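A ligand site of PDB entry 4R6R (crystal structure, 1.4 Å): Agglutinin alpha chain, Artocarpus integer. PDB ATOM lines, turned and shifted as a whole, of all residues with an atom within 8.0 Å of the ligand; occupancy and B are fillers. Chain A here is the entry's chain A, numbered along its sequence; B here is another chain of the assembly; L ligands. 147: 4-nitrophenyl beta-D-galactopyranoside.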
ATOM      1  N   GLY A   1      29.447  18.611 -11.105  1.00  0.00           N
ATOM      2  CA  GLY A   1      28.866  17.244 -11.348  1.00  0.00           C
ATOM      3  C   GLY A   1      27.862  17.339 -12.456  1.00  0.00           C
ATOM      4  O   GLY A   1      27.614  18.448 -12.977  1.00  0.00           O
ATOM      5  N   LYS A   2      27.356  16.190 -12.901  1.00  0.00           N
ATOM      6  CA  LYS A   2      26.351  16.139 -13.961  1.00  0.00           C
ATOM      7  C   LYS A   2      24.934  16.249 -13.345  1.00  0.00           C
ATOM      8  O   LYS A   2      24.515  15.391 -12.543  1.00  0.00           O
ATOM      9  CB  LYS A   2      26.472  14.859 -14.779  1.00  0.00           C
ATOM     10  CG  LYS A   2      25.442  14.702 -15.888  1.00  0.00           C
ATOM     11  CD  LYS A   2      25.640  13.423 -16.682  1.00  0.00           C
ATOM     12  CE  LYS A   2      24.789  13.460 -17.953  1.00  0.00           C
ATOM     13  NZ  LYS A   2      24.617  12.118 -18.615  1.00  0.00           N
ATOM     14  N   ALA A  24      30.940   8.750   0.577  1.00  0.00           N
ATOM     15  CA  ALA A  24      29.638   9.395   0.371  1.00  0.00           C
ATOM     16  C   ALA A  24      28.769   8.526  -0.564  1.00  0.00           C
ATOM     17  O   ALA A  24      29.169   7.400  -0.977  1.00  0.00           O
ATOM     18  CB  ALA A  24      29.875  10.804  -0.234  1.00  0.00           C
ATOM     19  N   ILE A  25      27.588   9.066  -0.902  1.00  0.00           N
ATOM     20  CA  ILE A  25      26.717   8.435  -1.887  1.00  0.00           C
ATOM     21  C   ILE A  25      27.288   8.623  -3.275  1.00  0.00           C
ATOM     22  O   ILE A  25      27.811   9.694  -3.641  1.00  0.00           O
ATOM     23  CB  ILE A  25      25.289   9.060  -1.805  1.00  0.00           C
ATOM     24  CG1 ILE A  25      24.764   8.990  -0.362  1.00  0.00           C
ATOM     25  CG2 ILE A  25      24.355   8.516  -2.897  1.00  0.00           C
ATOM     26  CD1 ILE A  25      24.478   7.537   0.043  1.00  0.00           C
ATOM     27  N   SER A  46      27.876   7.882 -10.692  1.00  0.00           N
ATOM     28  CA  SER A  46      29.143   8.528 -10.335  1.00  0.00           C
ATOM     29  C   SER A  46      30.130   8.418 -11.484  1.00  0.00           C
ATOM     30  O   SER A  46      30.125   7.425 -12.230  1.00  0.00           O
ATOM     31  CB  SER A  46      29.733   7.799  -9.125  1.00  0.00           C
ATOM     32  OG  SER A  46      31.014   8.288  -8.759  1.00  0.00           O
ATOM     33  N   PHE A  47      31.038   9.398 -11.497  1.00  0.00           N
ATOM     34  CA  PHE A  47      32.224   9.388 -12.410  1.00  0.00           C
ATOM     35  C   PHE A  47      33.244   8.360 -11.966  1.00  0.00           C
ATOM     36  O   PHE A  47      34.142   8.018 -12.771  1.00  0.00           O
ATOM     37  CB  PHE A  47      32.906  10.735 -12.404  1.00  0.00           C
ATOM     38  CG  PHE A  47      32.063  11.908 -12.868  1.00  0.00           C
ATOM     39  CD1 PHE A  47      30.851  11.749 -13.523  1.00  0.00           C
ATOM     40  CD2 PHE A  47      32.536  13.205 -12.653  1.00  0.00           C
ATOM     41  CE1 PHE A  47      30.117  12.874 -13.918  1.00  0.00           C
ATOM     42  CE2 PHE A  47      31.838  14.340 -13.066  1.00  0.00           C
ATOM     43  CZ  PHE A  47      30.618  14.158 -13.718  1.00  0.00           C
ATOM     44  N   ILE A  48      33.155   7.822 -10.760  1.00  0.00           N
ATOM     45  CA  ILE A  48      34.095   6.829 -10.234  1.00  0.00           C
ATOM     46  C   ILE A  48      33.475   5.507  -9.847  1.00  0.00           C
ATOM     47  O   ILE A  48      32.197   5.395  -9.731  1.00  0.00           O
ATOM     48  CB  ILE A  48      34.977   7.396  -9.074  1.00  0.00           C
ATOM     49  CG1 ILE A  48      34.145   7.616  -7.791  1.00  0.00           C
ATOM     50  CG2 ILE A  48      35.688   8.668  -9.487  1.00  0.00           C
ATOM     51  CD1 ILE A  48      34.993   8.185  -6.645  1.00  0.00           C
ATOM     52  N   VAL A  75      34.048  15.902   1.150  1.00  0.00           N
ATOM     53  CA  VAL A  75      34.857  14.802   0.653  1.00  0.00           C
ATOM     54  C   VAL A  75      35.751  15.361  -0.460  1.00  0.00           C
ATOM     55  O   VAL A  75      35.264  15.949  -1.395  1.00  0.00           O
ATOM     56  CB  VAL A  75      34.002  13.637   0.070  1.00  0.00           C
ATOM     57  CG1 VAL A  75      34.946  12.532  -0.433  1.00  0.00           C
ATOM     58  CG2 VAL A  75      33.060  13.054   1.127  1.00  0.00           C
ATOM     59  N   SER A  76      37.084  15.191  -0.341  1.00  0.00           N
ATOM     60  CA  SER A  76      38.062  15.639  -1.368  1.00  0.00           C
ATOM     61  C   SER A  76      37.877  17.147  -1.637  1.00  0.00           C
ATOM     62  O   SER A  76      38.130  17.634  -2.748  1.00  0.00           O
ATOM     63  CB  SER A  76      37.986  14.786  -2.627  1.00  0.00           C
ATOM     64  OG  SER A  76      38.391  13.459  -2.343  1.00  0.00           O
ATOM     65  N   GLY A  77      37.390  17.846  -0.619  1.00  0.00           N
ATOM     66  CA  GLY A  77      37.173  19.309  -0.691  1.00  0.00           C
ATOM     67  C   GLY A  77      35.914  19.762  -1.440  1.00  0.00           C
ATOM     68  O   GLY A  77      35.822  20.914  -1.904  1.00  0.00           O
ATOM     69  N   TYR A  78      34.974  18.836  -1.607  1.00  0.00           N
ATOM     70  CA  TYR A  78      33.668  19.154  -2.219  1.00  0.00           C
ATOM     71  C   TYR A  78      32.633  18.897  -1.128  1.00  0.00           C
ATOM     72  O   TYR A  78      32.768  17.928  -0.317  1.00  0.00           O
ATOM     73  CB  TYR A  78      33.393  18.208  -3.372  1.00  0.00           C
ATOM     74  CG  TYR A  78      34.309  18.398  -4.565  1.00  0.00           C
ATOM     75  CD1 TYR A  78      34.074  19.443  -5.464  1.00  0.00           C
ATOM     76  CD2 TYR A  78      35.415  17.577  -4.762  1.00  0.00           C
ATOM     77  CE1 TYR A  78      34.924  19.650  -6.573  1.00  0.00           C
ATOM     78  CE2 TYR A  78      36.249  17.762  -5.856  1.00  0.00           C
ATOM     79  CZ  TYR A  78      35.993  18.801  -6.752  1.00  0.00           C
ATOM     80  OH  TYR A  78      36.814  19.016  -7.854  1.00  0.00           O
ATOM     81  N   VAL A  79      31.627  19.753  -1.085  1.00  0.00           N
ATOM     82  CA  VAL A  79      30.478  19.450  -0.192  1.00  0.00           C
ATOM     83  C   VAL A  79      29.540  18.507  -0.937  1.00  0.00           C
ATOM     84  O   VAL A  79      29.146  18.779  -2.058  1.00  0.00           O
ATOM     85  CB  VAL A  79      29.690  20.738   0.168  1.00  0.00           C
ATOM     86  CG1 VAL A  79      28.435  20.389   0.993  1.00  0.00           C
ATOM     87  CG2 VAL A  79      30.606  21.776   0.848  1.00  0.00           C
ATOM     88  N   VAL A  80      29.308  17.341  -0.336  1.00  0.00           N
ATOM     89  CA  VAL A  80      28.511  16.270  -1.017  1.00  0.00           C
ATOM     90  C   VAL A  80      27.533  15.654   0.001  1.00  0.00           C
ATOM     91  O   VAL A  80      27.582  15.967   1.174  1.00  0.00           O
ATOM     92  CB  VAL A  80      29.433  15.187  -1.667  1.00  0.00           C
ATOM     93  CG1 VAL A  80      30.377  15.851  -2.680  1.00  0.00           C
ATOM     94  CG2 VAL A  80      30.263  14.476  -0.597  1.00  0.00           C
ATOM     95  N   VAL A  81      26.590  14.831  -0.486  1.00  0.00           N
ATOM     96  CA  VAL A  81      25.687  14.124   0.377  1.00  0.00           C
ATOM     97  C   VAL A  81      26.441  12.847   0.801  1.00  0.00           C
ATOM     98  O   VAL A  81      26.655  11.927   0.010  1.00  0.00           O
ATOM     99  CB  VAL A  81      24.422  13.763  -0.397  1.00  0.00           C
ATOM    100  CG1 VAL A  81      23.457  12.972   0.485  1.00  0.00           C
ATOM    101  CG2 VAL A  81      23.811  15.065  -0.871  1.00  0.00           C
ATOM    102  N   SER A 119      22.517  16.444  -8.638  1.00  0.00           N
ATOM    103  CA  SER A 119      23.729  16.453  -9.467  1.00  0.00           C
ATOM    104  C   SER A 119      24.700  15.439  -8.854  1.00  0.00           C
ATOM    105  O   SER A 119      24.771  15.344  -7.628  1.00  0.00           O
ATOM    106  CB  SER A 119      24.367  17.846  -9.373  1.00  0.00           C
ATOM    107  OG  SER A 119      25.589  17.875 -10.095  1.00  0.00           O
ATOM    108  N   ILE A 120      25.376  14.652  -9.727  1.00  0.00           N
ATOM    109  CA  ILE A 120      26.361  13.670  -9.256  1.00  0.00           C
ATOM    110  C   ILE A 120      27.632  13.903 -10.088  1.00  0.00           C
ATOM    111  O   ILE A 120      27.598  13.862 -11.309  1.00  0.00           O
ATOM    112  CB  ILE A 120      25.832  12.242  -9.457  1.00  0.00           C
ATOM    113  CG1 ILE A 120      24.532  12.099  -8.684  1.00  0.00           C
ATOM    114  CG2 ILE A 120      26.820  11.195  -8.942  1.00  0.00           C
ATOM    115  CD1 ILE A 120      23.897  10.736  -8.811  1.00  0.00           C
ATOM    116  N   GLY A 121      28.710  14.029  -9.317  1.00  0.00           N
ATOM    117  CA  GLY A 121      30.071  14.112  -9.917  1.00  0.00           C
ATOM    118  C   GLY A 121      30.812  12.841  -9.485  1.00  0.00           C
ATOM    119  O   GLY A 121      30.385  11.706  -9.771  1.00  0.00           O
ATOM    120  N   TYR A 122      31.910  12.960  -8.710  1.00  0.00           N
ATOM    121  CA  TYR A 122      32.452  11.748  -8.044  1.00  0.00           C
ATOM    122  C   TYR A 122      31.374  11.202  -7.073  1.00  0.00           C
ATOM    123  O   TYR A 122      31.254   9.986  -6.846  1.00  0.00           O
ATOM    124  CB  TYR A 122      33.745  12.096  -7.261  1.00  0.00           C
ATOM    125  CG  TYR A 122      35.013  12.215  -8.138  1.00  0.00           C
ATOM    126  CD1 TYR A 122      34.933  12.481  -9.479  1.00  0.00           C
ATOM    127  CD2 TYR A 122      36.259  11.914  -7.598  1.00  0.00           C
ATOM    128  CE1 TYR A 122      36.063  12.575 -10.293  1.00  0.00           C
ATOM    129  CE2 TYR A 122      37.401  11.961  -8.404  1.00  0.00           C
ATOM    130  CZ  TYR A 122      37.273  12.291  -9.717  1.00  0.00           C
ATOM    131  OH  TYR A 122      38.394  12.351 -10.544  1.00  0.00           O
ATOM    132  N   TRP A 123      30.714  12.157  -6.407  1.00  0.00           N
ATOM    133  CA  TRP A 123      29.650  11.789  -5.410  1.00  0.00           C
ATOM    134  C   TRP A 123      28.381  12.587  -5.728  1.00  0.00           C
ATOM    135  O   TRP A 123      28.371  13.543  -6.518  1.00  0.00           O
ATOM    136  CB  TRP A 123      30.077  11.984  -3.939  1.00  0.00           C
ATOM    137  CG  TRP A 123      31.361  11.235  -3.737  1.00  0.00           C
ATOM    138  CD1 TRP A 123      31.514   9.854  -3.612  1.00  0.00           C
ATOM    139  CD2 TRP A 123      32.706  11.810  -3.800  1.00  0.00           C
ATOM    140  NE1 TRP A 123      32.881   9.563  -3.557  1.00  0.00           N
ATOM    141  CE2 TRP A 123      33.621  10.702  -3.641  1.00  0.00           C
ATOM    142  CE3 TRP A 123      33.224  13.101  -3.999  1.00  0.00           C
ATOM    143  CZ2 TRP A 123      35.034  10.881  -3.680  1.00  0.00           C
ATOM    144  CZ3 TRP A 123      34.634  13.266  -3.982  1.00  0.00           C
ATOM    145  CH2 TRP A 123      35.493  12.173  -3.834  1.00  0.00           C
ATOM    146  N   LEU A 124      27.279  12.190  -5.049  1.00  0.00           N
ATOM    147  CA  LEU A 124      26.032  12.955  -5.093  1.00  0.00           C
ATOM    148  C   LEU A 124      26.333  14.327  -4.450  1.00  0.00           C
ATOM    149  O   LEU A 124      26.600  14.440  -3.273  1.00  0.00           O
ATOM    150  CB  LEU A 124      24.965  12.194  -4.292  1.00  0.00           C
ATOM    151  CG  LEU A 124      23.555  12.893  -4.223  1.00  0.00           C
ATOM    152  CD1 LEU A 124      22.965  13.142  -5.594  1.00  0.00           C
ATOM    153  CD2 LEU A 124      22.643  12.019  -3.332  1.00  0.00           C
ATOM    154  N   ASP A 125      26.229  15.352  -5.274  1.00  0.00           N
ATOM    155  CA  ASP A 125      26.552  16.700  -4.818  1.00  0.00           C
ATOM    156  C   ASP A 125      25.413  17.325  -4.048  1.00  0.00           C
ATOM    157  O   ASP A 125      25.638  17.942  -3.039  1.00  0.00           O
ATOM    158  CB  ASP A 125      26.864  17.621  -6.024  1.00  0.00           C
ATOM    159  CG  ASP A 125      28.018  17.080  -6.909  1.00  0.00           C
ATOM    160  OD1 ASP A 125      29.079  16.819  -6.302  1.00  0.00           O
ATOM    161  OD2 ASP A 125      27.814  16.880  -8.146  1.00  0.00           O
ATOM    162  N   TYR A 126      24.188  17.145  -4.569  1.00  0.00           N
ATOM    163  CA  TYR A 126      23.033  17.780  -3.927  1.00  0.00           C
ATOM    164  C   TYR A 126      21.860  17.064  -4.560  1.00  0.00           C
ATOM    165  O   TYR A 126      21.965  16.458  -5.645  1.00  0.00           O
ATOM    166  CB  TYR A 126      22.990  19.349  -4.114  1.00  0.00           C
ATOM    167  CG  TYR A 126      22.949  19.812  -5.513  1.00  0.00           C
ATOM    168  CD1 TYR A 126      21.775  19.747  -6.277  1.00  0.00           C
ATOM    169  CD2 TYR A 126      24.118  20.360  -6.123  1.00  0.00           C
ATOM    170  CE1 TYR A 126      21.764  20.143  -7.607  1.00  0.00           C
ATOM    171  CE2 TYR A 126      24.115  20.767  -7.448  1.00  0.00           C
ATOM    172  CZ  TYR A 126      22.952  20.666  -8.189  1.00  0.00           C
ATOM    173  OH  TYR A 126      22.977  21.094  -9.504  1.00  0.00           O
ATOM    174  N   ALA B  16      25.760  20.504  -1.783  1.00  0.00           N
ATOM    175  CA  ALA B  16      26.538  21.620  -2.271  1.00  0.00           C
ATOM    176  C   ALA B  16      25.608  22.755  -2.723  1.00  0.00           C
ATOM    177  O   ALA B  16      24.531  22.512  -3.285  1.00  0.00           O
ATOM    178  CB  ALA B  16      27.368  21.170  -3.413  1.00  0.00           C
HETATM  179  C1  147 L   1      33.899  16.521  -9.504  1.00  0.00           C
HETATM  180  C2  147 L   1      33.136  17.685 -10.178  1.00  0.00           C
HETATM  181  O2  147 L   1      33.960  18.460 -11.099  1.00  0.00           O
HETATM  182  C3  147 L   1      32.546  18.648  -9.132  1.00  0.00           C
HETATM  183  O3  147 L   1      31.680  19.585  -9.812  1.00  0.00           O
HETATM  184  C4  147 L   1      31.725  17.792  -8.049  1.00  0.00           C
HETATM  185  O4  147 L   1      30.649  17.254  -8.787  1.00  0.00           O
HETATM  186  C5  147 L   1      32.656  16.613  -7.496  1.00  0.00           C
HETATM  187  C6  147 L   1      32.132  15.918  -6.215  1.00  0.00           C
HETATM  188  O6  147 L   1      31.082  14.977  -6.494  1.00  0.00           O
HETATM  189  O5  147 L   1      33.044  15.712  -8.561  1.00  0.00           O
HETATM  190  O1  147 L   1      34.521  15.760 -10.563  1.00  0.00           O
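N of Ala 16 of chain B lies within hydrogen-bond range of O of Asp 125. N of Phe 47 is in hydrogen-bond range of O of Gly 121, 3.0 Å away. The backbone NH (N) of Asp 125 sits at hydrogen-bond distance from the backbone carbonyl oxygen (O) of Ser 119 (2.8 Å). OD2 of Asp 125 sits at hydrogen-bond distance from N of Gly 121 (3.2 Å). The side-chain hydroxyl of Ser 46 sits at hydrogen-bond distance from the backbone carbonyl oxygen of Tyr 122 (2.6 Å).
Phe 47 touches the ligand (CD2 to O1, 3.9 Å). Tyr 78 touches the ligand (CE1 to C3, 3.6 Å). Val 80 touches the ligand. CA of Gly 121 touches O4 of the ligand (3.4 Å). Of the 23 residues printed, 8 come within 4 Å of the ligand. Along chain A the residues within 4 Å of the ligand span positions 1 to 125.
The backbone NH of Tyr 122 is in hydrogen-bond range of an oxygen (O5) of the ligand (3.0 Å). The backbone carbonyl oxygen of Trp 123 is in hydrogen-bond range of an oxygen (O6) of the ligand (3.1 Å). N of Trp 123 lies within hydrogen-bond range of O6 of the ligand (2.8 Å). OD1 of Asp 125 sits at hydrogen-bond distance from O6 of the ligand (2.7 Å). O3 of the ligand sits at hydrogen-bond distance from N of Gly 1 (2.8 Å).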
